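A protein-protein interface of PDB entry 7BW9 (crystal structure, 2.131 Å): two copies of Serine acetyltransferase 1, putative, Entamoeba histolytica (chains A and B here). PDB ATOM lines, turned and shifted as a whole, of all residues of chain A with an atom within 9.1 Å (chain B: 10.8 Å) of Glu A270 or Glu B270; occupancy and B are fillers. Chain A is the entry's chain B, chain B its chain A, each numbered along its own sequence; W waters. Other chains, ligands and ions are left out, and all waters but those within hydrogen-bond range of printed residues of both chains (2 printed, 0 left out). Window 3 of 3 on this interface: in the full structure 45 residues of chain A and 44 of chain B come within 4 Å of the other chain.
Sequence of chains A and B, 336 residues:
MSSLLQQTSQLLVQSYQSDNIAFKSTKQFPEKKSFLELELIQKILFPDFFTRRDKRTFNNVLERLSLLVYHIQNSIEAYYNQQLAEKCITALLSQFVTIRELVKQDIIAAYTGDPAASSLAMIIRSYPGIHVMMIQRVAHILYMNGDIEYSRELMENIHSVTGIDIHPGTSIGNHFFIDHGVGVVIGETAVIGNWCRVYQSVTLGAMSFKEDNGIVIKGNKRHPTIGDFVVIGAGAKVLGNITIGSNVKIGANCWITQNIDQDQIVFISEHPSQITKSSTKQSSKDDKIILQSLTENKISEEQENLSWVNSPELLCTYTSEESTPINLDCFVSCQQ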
ATOM      1  N   ASN A 253     -20.663 -13.221 -19.369  1.00  0.00           N
ATOM      2  CA  ASN A 253     -20.259 -12.320 -18.286  1.00  0.00           C
ATOM      3  C   ASN A 253     -18.763 -12.010 -18.231  1.00  0.00           C
ATOM      4  O   ASN A 253     -18.321 -11.367 -17.278  1.00  0.00           O
ATOM      5  CB  ASN A 253     -20.730 -12.839 -16.915  1.00  0.00           C
ATOM      6  CG  ASN A 253     -22.178 -12.448 -16.630  1.00  0.00           C
ATOM      7  OD1 ASN A 253     -22.815 -11.818 -17.458  1.00  0.00           O
ATOM      8  ND2 ASN A 253     -22.695 -12.813 -15.468  1.00  0.00           N
ATOM      9  N   CYS A 254     -17.974 -12.393 -19.231  1.00  0.00           N
ATOM     10  CA  CYS A 254     -16.569 -11.995 -19.232  1.00  0.00           C
ATOM     11  C   CYS A 254     -16.416 -10.480 -19.270  1.00  0.00           C
ATOM     12  O   CYS A 254     -17.176  -9.765 -19.936  1.00  0.00           O
ATOM     13  CB  CYS A 254     -15.823 -12.571 -20.431  1.00  0.00           C
ATOM     14  SG  CYS A 254     -15.469 -14.295 -20.368  1.00  0.00           S
ATOM     15  N   TRP A 255     -15.399  -9.992 -18.589  1.00  0.00           N
ATOM     16  CA  TRP A 255     -14.999  -8.596 -18.698  1.00  0.00           C
ATOM     17  C   TRP A 255     -13.714  -8.598 -19.499  1.00  0.00           C
ATOM     18  O   TRP A 255     -12.704  -9.138 -19.051  1.00  0.00           O
ATOM     19  CB  TRP A 255     -14.819  -7.966 -17.325  1.00  0.00           C
ATOM     20  CG  TRP A 255     -14.272  -6.589 -17.331  1.00  0.00           C
ATOM     21  CD1 TRP A 255     -14.744  -5.512 -18.028  1.00  0.00           C
ATOM     22  CD2 TRP A 255     -13.152  -6.120 -16.572  1.00  0.00           C
ATOM     23  NE1 TRP A 255     -13.981  -4.401 -17.749  1.00  0.00           N
ATOM     24  CE2 TRP A 255     -12.997  -4.752 -16.857  1.00  0.00           C
ATOM     25  CE3 TRP A 255     -12.263  -6.730 -15.677  1.00  0.00           C
ATOM     26  CZ2 TRP A 255     -11.981  -3.982 -16.286  1.00  0.00           C
ATOM     27  CZ3 TRP A 255     -11.263  -5.967 -15.108  1.00  0.00           C
ATOM     28  CH2 TRP A 255     -11.128  -4.609 -15.414  1.00  0.00           C
ATOM     29  N   ILE A 256     -13.761  -8.038 -20.700  1.00  0.00           N
ATOM     30  CA  ILE A 256     -12.673  -8.177 -21.657  1.00  0.00           C
ATOM     31  C   ILE A 256     -12.156  -6.793 -22.011  1.00  0.00           C
ATOM     32  O   ILE A 256     -12.872  -5.983 -22.618  1.00  0.00           O
ATOM     33  CB  ILE A 256     -13.117  -8.953 -22.899  1.00  0.00           C
ATOM     34  CG1 ILE A 256     -13.247 -10.427 -22.521  1.00  0.00           C
ATOM     35  CG2 ILE A 256     -12.139  -8.756 -24.048  1.00  0.00           C
ATOM     36  CD1 ILE A 256     -13.680 -11.282 -23.629  1.00  0.00           C
ATOM     37  N   THR A 257     -10.909  -6.521 -21.631  1.00  0.00           N
ATOM     38  CA  THR A 257     -10.283  -5.236 -21.900  1.00  0.00           C
ATOM     39  C   THR A 257      -8.956  -5.385 -22.628  1.00  0.00           C
ATOM     40  O   THR A 257      -8.210  -4.410 -22.718  1.00  0.00           O
ATOM     41  CB  THR A 257     -10.076  -4.442 -20.596  1.00  0.00           C
ATOM     42  OG1 THR A 257      -9.330  -5.230 -19.650  1.00  0.00           O
ATOM     43  CG2 THR A 257     -11.419  -4.061 -19.979  1.00  0.00           C
ATOM     44  N   GLN A 258      -8.644  -6.571 -23.151  1.00  0.00           N
ATOM     45  CA  GLN A 258      -7.385  -6.830 -23.837  1.00  0.00           C
ATOM     46  C   GLN A 258      -7.640  -7.424 -25.212  1.00  0.00           C
ATOM     47  O   GLN A 258      -8.628  -8.135 -25.420  1.00  0.00           O
ATOM     48  CB  GLN A 258      -6.494  -7.830 -23.071  1.00  0.00           C
ATOM     49  CG  GLN A 258      -6.532  -7.743 -21.574  1.00  0.00           C
ATOM     50  CD  GLN A 258      -5.571  -8.731 -20.927  1.00  0.00           C
ATOM     51  OE1 GLN A 258      -5.589  -9.934 -21.213  1.00  0.00           O
ATOM     52  NE2 GLN A 258      -4.716  -8.222 -20.062  1.00  0.00           N
ATOM     53  N   PHE A 267     -13.189 -17.303 -20.967  1.00  0.00           N
ATOM     54  CA  PHE A 267     -14.224 -17.625 -19.995  1.00  0.00           C
ATOM     55  C   PHE A 267     -13.755 -17.182 -18.623  1.00  0.00           C
ATOM     56  O   PHE A 267     -12.553 -17.085 -18.358  1.00  0.00           O
ATOM     57  CB  PHE A 267     -14.571 -19.123 -19.990  1.00  0.00           C
ATOM     58  CG  PHE A 267     -13.376 -20.022 -19.809  1.00  0.00           C
ATOM     59  CD1 PHE A 267     -12.552 -20.332 -20.883  1.00  0.00           C
ATOM     60  CD2 PHE A 267     -13.066 -20.548 -18.561  1.00  0.00           C
ATOM     61  CE1 PHE A 267     -11.441 -21.153 -20.723  1.00  0.00           C
ATOM     62  CE2 PHE A 267     -11.949 -21.381 -18.386  1.00  0.00           C
ATOM     63  CZ  PHE A 267     -11.142 -21.681 -19.467  1.00  0.00           C
ATOM     64  N   ILE A 268     -14.727 -16.911 -17.752  1.00  0.00           N
ATOM     65  CA  ILE A 268     -14.400 -16.512 -16.392  1.00  0.00           C
ATOM     66  C   ILE A 268     -13.598 -17.622 -15.732  1.00  0.00           C
ATOM     67  O   ILE A 268     -13.936 -18.809 -15.839  1.00  0.00           O
ATOM     68  CB  ILE A 268     -15.681 -16.172 -15.622  1.00  0.00           C
ATOM     69  CG1 ILE A 268     -16.281 -14.883 -16.188  1.00  0.00           C
ATOM     70  CG2 ILE A 268     -15.396 -16.017 -14.133  1.00  0.00           C
ATOM     71  CD1 ILE A 268     -17.662 -14.583 -15.651  1.00  0.00           C
ATOM     72  N   SER A 269     -12.514 -17.235 -15.060  1.00  0.00           N
ATOM     73  CA  SER A 269     -11.518 -18.197 -14.601  1.00  0.00           C
ATOM     74  C   SER A 269     -12.135 -19.284 -13.727  1.00  0.00           C
ATOM     75  O   SER A 269     -12.122 -20.469 -14.083  1.00  0.00           O
ATOM     76  CB  SER A 269     -10.403 -17.461 -13.851  1.00  0.00           C
ATOM     77  OG  SER A 269     -10.133 -16.196 -14.442  1.00  0.00           O
ATOM     78  N   GLU A 270     -12.694 -18.903 -12.583  1.00  0.00           N
ATOM     79  CA  GLU A 270     -13.106 -19.897 -11.604  1.00  0.00           C
ATOM     80  C   GLU A 270     -14.583 -19.787 -11.247  1.00  0.00           C
ATOM     81  O   GLU A 270     -15.218 -18.732 -11.372  1.00  0.00           O
ATOM     82  CB  GLU A 270     -12.263 -19.803 -10.327  1.00  0.00           C
ATOM     83  CG  GLU A 270     -10.927 -20.526 -10.433  1.00  0.00           C
ATOM     84  CD  GLU A 270      -9.791 -19.595 -10.812  1.00  0.00           C
ATOM     85  OE1 GLU A 270      -9.841 -18.405 -10.420  1.00  0.00           O
ATOM     86  OE2 GLU A 270      -8.858 -20.049 -11.510  1.00  0.00           O
ATOM     87  N   HIS A 271     -15.107 -20.924 -10.778  1.00  0.00           N
ATOM     88  CA  HIS A 271     -16.476 -21.027 -10.311  1.00  0.00           C
ATOM     89  C   HIS A 271     -16.686 -20.179  -9.053  1.00  0.00           C
ATOM     90  O   HIS A 271     -15.725 -19.755  -8.401  1.00  0.00           O
ATOM     91  CB  HIS A 271     -16.815 -22.492 -10.026  1.00  0.00           C
ATOM     92  CG  HIS A 271     -16.962 -23.333 -11.257  1.00  0.00           C
ATOM     93  ND1 HIS A 271     -17.517 -22.855 -12.427  1.00  0.00           N
ATOM     94  CD2 HIS A 271     -16.630 -24.625 -11.499  1.00  0.00           C
ATOM     95  CE1 HIS A 271     -17.522 -23.816 -13.335  1.00  0.00           C
ATOM     96  NE2 HIS A 271     -16.989 -24.900 -12.798  1.00  0.00           N
ATOM     97  N   PRO A 272     -17.939 -19.903  -8.708  1.00  0.00           N
ATOM     98  CA  PRO A 272     -18.248 -19.177  -7.472  1.00  0.00           C
ATOM     99  C   PRO A 272     -18.298 -20.096  -6.250  1.00  0.00           C
ATOM    100  O   PRO A 272     -18.140 -21.313  -6.336  1.00  0.00           O
ATOM    101  CB  PRO A 272     -19.618 -18.563  -7.772  1.00  0.00           C
ATOM    102  CG  PRO A 272     -20.218 -19.440  -8.802  1.00  0.00           C
ATOM    103  CD  PRO A 272     -19.079 -19.912  -9.644  1.00  0.00           C
ATOM    104  N   SER A 273     -18.528 -19.478  -5.094  1.00  0.00           N
ATOM    105  CA  SER A 273     -18.626 -20.175  -3.821  1.00  0.00           C
ATOM    106  C   SER A 273     -20.035 -20.703  -3.574  1.00  0.00           C
ATOM    107  O   SER A 273     -21.028 -20.111  -4.001  1.00  0.00           O
ATOM    108  CB  SER A 273     -18.246 -19.235  -2.677  1.00  0.00           C
ATOM    109  OG  SER A 273     -16.881 -19.367  -2.347  1.00  0.00           O
ATOM    110  N   ALA B 252     -16.530  -2.247 -15.109  1.00  0.00           N
ATOM    111  CA  ALA B 252     -17.626  -3.043 -15.643  1.00  0.00           C
ATOM    112  C   ALA B 252     -17.763  -4.379 -14.921  1.00  0.00           C
ATOM    113  O   ALA B 252     -16.774  -4.978 -14.510  1.00  0.00           O
ATOM    114  CB  ALA B 252     -17.411  -3.285 -17.136  1.00  0.00           C
ATOM    115  N   ASN B 253     -19.007  -4.829 -14.759  1.00  0.00           N
ATOM    116  CA  ASN B 253     -19.378  -6.145 -14.244  1.00  0.00           C
ATOM    117  C   ASN B 253     -18.994  -6.366 -12.784  1.00  0.00           C
ATOM    118  O   ASN B 253     -19.148  -7.481 -12.283  1.00  0.00           O
ATOM    119  CB  ASN B 253     -18.793  -7.276 -15.110  1.00  0.00           C
ATOM    120  CG  ASN B 253     -19.617  -7.513 -16.345  1.00  0.00           C
ATOM    121  OD1 ASN B 253     -20.647  -6.851 -16.541  1.00  0.00           O
ATOM    122  ND2 ASN B 253     -19.189  -8.451 -17.189  1.00  0.00           N
ATOM    123  N   CYS B 254     -18.537  -5.332 -12.079  1.00  0.00           N
ATOM    124  CA  CYS B 254     -18.249  -5.464 -10.653  1.00  0.00           C
ATOM    125  C   CYS B 254     -19.487  -5.852  -9.854  1.00  0.00           C
ATOM    126  O   CYS B 254     -20.617  -5.465 -10.170  1.00  0.00           O
ATOM    127  CB  CYS B 254     -17.694  -4.156 -10.093  1.00  0.00           C
ATOM    128  SG  CYS B 254     -15.937  -3.958 -10.393  1.00  0.00           S
ATOM    129  N   VAL B 266     -12.344   0.805  -8.457  1.00  0.00           N
ATOM    130  CA  VAL B 266     -12.741  -0.591  -8.118  1.00  0.00           C
ATOM    131  C   VAL B 266     -12.896  -1.389  -9.410  1.00  0.00           C
ATOM    132  O   VAL B 266     -13.526  -0.892 -10.340  1.00  0.00           O
ATOM    133  CB  VAL B 266     -14.030  -0.605  -7.286  1.00  0.00           C
ATOM    134  CG1 VAL B 266     -14.387  -1.992  -6.808  1.00  0.00           C
ATOM    135  CG2 VAL B 266     -13.955   0.360  -6.123  1.00  0.00           C
ATOM    136  N   PHE B 267     -12.372  -2.608  -9.421  1.00  0.00           N
ATOM    137  CA  PHE B 267     -12.403  -3.446 -10.641  1.00  0.00           C
ATOM    138  C   PHE B 267     -12.333  -4.926 -10.265  1.00  0.00           C
ATOM    139  O   PHE B 267     -11.827  -5.261  -9.188  1.00  0.00           O
ATOM    140  CB  PHE B 267     -11.200  -3.081 -11.511  1.00  0.00           C
ATOM    141  CG  PHE B 267      -9.894  -3.062 -10.762  1.00  0.00           C
ATOM    142  CD1 PHE B 267      -9.511  -1.955 -10.021  1.00  0.00           C
ATOM    143  CD2 PHE B 267      -9.062  -4.165 -10.761  1.00  0.00           C
ATOM    144  CE1 PHE B 267      -8.318  -1.945  -9.319  1.00  0.00           C
ATOM    145  CE2 PHE B 267      -7.875  -4.161 -10.048  1.00  0.00           C
ATOM    146  CZ  PHE B 267      -7.500  -3.051  -9.332  1.00  0.00           C
ATOM    147  N   ILE B 268     -12.788  -5.784 -11.178  1.00  0.00           N
ATOM    148  CA  ILE B 268     -12.710  -7.263 -10.995  1.00  0.00           C
ATOM    149  C   ILE B 268     -11.224  -7.636 -10.860  1.00  0.00           C
ATOM    150  O   ILE B 268     -10.407  -7.103 -11.613  1.00  0.00           O
ATOM    151  CB  ILE B 268     -13.459  -7.990 -12.128  1.00  0.00           C
ATOM    152  CG1 ILE B 268     -14.963  -7.700 -12.053  1.00  0.00           C
ATOM    153  CG2 ILE B 268     -13.162  -9.480 -12.101  1.00  0.00           C
ATOM    154  CD1 ILE B 268     -15.681  -7.735 -13.372  1.00  0.00           C
ATOM    155  N   SER B 269     -10.906  -8.558  -9.958  1.00  0.00           N
ATOM    156  CA  SER B 269      -9.510  -8.842  -9.609  1.00  0.00           C
ATOM    157  C   SER B 269      -8.737  -9.495 -10.746  1.00  0.00           C
ATOM    158  O   SER B 269      -7.517  -9.319 -10.841  1.00  0.00           O
ATOM    159  CB  SER B 269      -9.434  -9.748  -8.373  1.00  0.00           C
ATOM    160  OG  SER B 269     -10.205  -9.232  -7.296  1.00  0.00           O
ATOM    161  N   GLU B 270      -9.413 -10.252 -11.605  1.00  0.00           N
ATOM    162  CA  GLU B 270      -8.751 -11.201 -12.488  1.00  0.00           C
ATOM    163  C   GLU B 270      -9.350 -11.141 -13.889  1.00  0.00           C
ATOM    164  O   GLU B 270     -10.572 -11.073 -14.048  1.00  0.00           O
ATOM    165  CB  GLU B 270      -8.878 -12.625 -11.920  1.00  0.00           C
ATOM    166  CG  GLU B 270      -8.126 -13.692 -12.688  1.00  0.00           C
ATOM    167  CD  GLU B 270      -8.043 -15.010 -11.921  1.00  0.00           C
ATOM    168  OE1 GLU B 270      -8.136 -14.991 -10.670  1.00  0.00           O
ATOM    169  OE2 GLU B 270      -7.892 -16.067 -12.571  1.00  0.00           O
ATOM    170  N   HIS B 271      -8.483 -11.159 -14.901  1.00  0.00           N
ATOM    171  CA  HIS B 271      -8.952 -11.322 -16.270  1.00  0.00           C
ATOM    172  C   HIS B 271      -9.531 -12.723 -16.454  1.00  0.00           C
ATOM    173  O   HIS B 271      -9.166 -13.657 -15.734  1.00  0.00           O
ATOM    174  CB  HIS B 271      -7.823 -11.119 -17.282  1.00  0.00           C
ATOM    175  CG  HIS B 271      -7.271  -9.729 -17.314  1.00  0.00           C
ATOM    176  ND1 HIS B 271      -7.772  -8.745 -18.140  1.00  0.00           N
ATOM    177  CD2 HIS B 271      -6.251  -9.161 -16.628  1.00  0.00           C
ATOM    178  CE1 HIS B 271      -7.083  -7.630 -17.964  1.00  0.00           C
ATOM    179  NE2 HIS B 271      -6.152  -7.857 -17.053  1.00  0.00           N
ATOM    180  N   PRO B 272     -10.445 -12.894 -17.399  1.00  0.00           N
ATOM    181  CA  PRO B 272     -10.898 -14.243 -17.731  1.00  0.00           C
ATOM    182  C   PRO B 272      -9.740 -15.071 -18.258  1.00  0.00           C
ATOM    183  O   PRO B 272      -8.748 -14.551 -18.772  1.00  0.00           O
ATOM    184  CB  PRO B 272     -11.961 -14.017 -18.813  1.00  0.00           C
ATOM    185  CG  PRO B 272     -11.730 -12.628 -19.310  1.00  0.00           C
ATOM    186  CD  PRO B 272     -11.156 -11.859 -18.171  1.00  0.00           C
ATOM    187  N   SER B 273      -9.877 -16.378 -18.120  1.00  0.00           N
ATOM    188  CA  SER B 273      -8.874 -17.274 -18.662  1.00  0.00           C
ATOM    189  C   SER B 273      -9.181 -17.602 -20.125  1.00  0.00           C
ATOM    190  O   SER B 273     -10.264 -17.322 -20.656  1.00  0.00           O
ATOM    191  CB  SER B 273      -8.762 -18.532 -17.799  1.00  0.00           C
ATOM    192  OG  SER B 273     -10.027 -18.947 -17.322  1.00  0.00           O
ATOM    193  N   GLN B 274      -8.201 -18.222 -20.769  1.00  0.00           N
ATOM    194  CA  GLN B 274      -8.044 -18.150 -22.217  1.00  0.00           C
ATOM    195  C   GLN B 274      -7.335 -19.414 -22.683  1.00  0.00           C
ATOM    196  O   GLN B 274      -6.204 -19.671 -22.260  1.00  0.00           O
ATOM    197  CB  GLN B 274      -7.234 -16.896 -22.559  1.00  0.00           C
ATOM    198  CG  GLN B 274      -7.304 -16.382 -23.971  1.00  0.00           C
ATOM    199  CD  GLN B 274      -6.820 -14.942 -24.062  1.00  0.00           C
ATOM    200  OE1 GLN B 274      -6.984 -14.159 -23.123  1.00  0.00           O
ATOM    201  NE2 GLN B 274      -6.213 -14.586 -25.192  1.00  0.00           N
HETATM  202  O   HOH W   1      -9.676  -9.040 -20.407  1.00  0.00           O
HETATM  203  O   HOH W   2     -14.100  -0.948 -17.221  1.00  0.00           O
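Water W1 lies within hydrogen-bond range of a ring nitrogen (ND1) of His B271 (3.0 Å), the backbone NH of Thr A257 (3.1 Å) and the backbone carbonyl oxygen of Trp A255 (3.3 Å). Water W2 bridges the backbone NH of Ala B252 (3.5 Å) and the indole nitrogen of Trp A255 (3.5 Å).
Of chain B, only Glu B270 comes within 4 Å of Glu A270. Of chain A, only Ser A269 and Glu A270 come within 4 Å of Glu B270. Ile A268 touches none of the printed residues of chain B. Of the printed residues of chain B, Ser A269 touches Glu B270 (2.9 Å), His B271 (3.0 Å), Pro B272 (3.9 Å) and Ser B273 (3.2 Å). No residue of chain B comes within 4 Å of His A271. No residue of chain B comes within 4 Å of Pro A272. No residue of chain A comes within 4 Å of Ser B269. Of the printed residues of chain A, Pro B272 touches Cys A254 (3.8 Å), Trp A255 (3.3 Å), Phe A267 (3.2 Å) and Ser A269 (3.9 Å). Printed residues of chain A within 4 Å of Asn B253: Asn A253 (3.0 Å) and Cys A254 (3.7 Å). Printed residues of chain A within 4 Å of Ile B268: Trp A255 (3.8 Å). Ile A256 touches none of the printed residues of chain B.
O of Cys A254 touches ND2 of Asn B253 (3.7 Å). Cys A254 touches Pro B272. Trp A255 touches Ala B252. Ile B268 touches Trp A255 (O to CZ3, 3.8 Å). O of Trp A255 touches CD of Pro B272, 3.3 Å away. OG1 of Thr A257 touches CE1 of His B271 (3.7 Å). CB of Pro B272 touches O of Phe A267 (3.2 Å). Pro B272 touches Ser A269. CA of Ser A269 touches OG of Ser B273 (3.2 Å). OE2 of Glu B270 touches OE1 of Glu A270 (3.7 Å).
Printed residues of chain A that touch a printed residue of chain B: Asn A253, Cys A254, Trp A255, Thr A257, Gln A258, Phe A267, Ser A269 and Glu A270. Printed residues of chain B that touch a printed residue of chain A: Ala B252, Asn B253, Ile B268, Glu B270, His B271, Pro B272 and Ser B273. Hydrophobic or aromatic side chains of chain B that line the printed part of chain A: Ala B252, Ile B268, His B271 and Pro B272. Along chain B the printed residues that touch a printed residue of chain A span positions 252 to 273.
The side-chain sulfur (SG) of Cys B254 sits at hydrogen-bond distance from the backbone NH (N) of Ile B268. N of Ile A268 lies within hydrogen-bond range of SG of Cys A254 (3.8 Å).
Ser A269 touches Glu B270, but with the chains exchanged Glu A270 does not touch Ser B269 (8.9 Å). Ser A269 touches His B271, but with the chains exchanged His A271 does not touch Ser B269 (11.8 Å). Ser A269 touches Pro B272, but with the chains exchanged Pro A272 does not touch Ser B269 (12.8 Å). Glu A270 touches its own counterpart, Glu B270. Positions printed for both chains: 253, 254, 267, 268, 269, 270, 271, 272 and 273.
ND2 of Asn B253 lies within hydrogen-bond range of O of Asn A253, 3.0 Å away. The side-chain carboxylate of Glu B270 lies within hydrogen-bond range of the side-chain hydroxyl of Ser A269, 2.9 Å away. A ring nitrogen (NE2) of His B271 sits close to the side-chain amide nitrogen (NE2) of Gln A258, 3.4 Å away. OG of Ser A269 lies within hydrogen-bond range of O of His B271, 3.0 Å away. The backbone NH (N) of Ser B273 sits at hydrogen-bond distance from the backbone carbonyl oxygen (O) of Phe A267 (2.8 Å).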
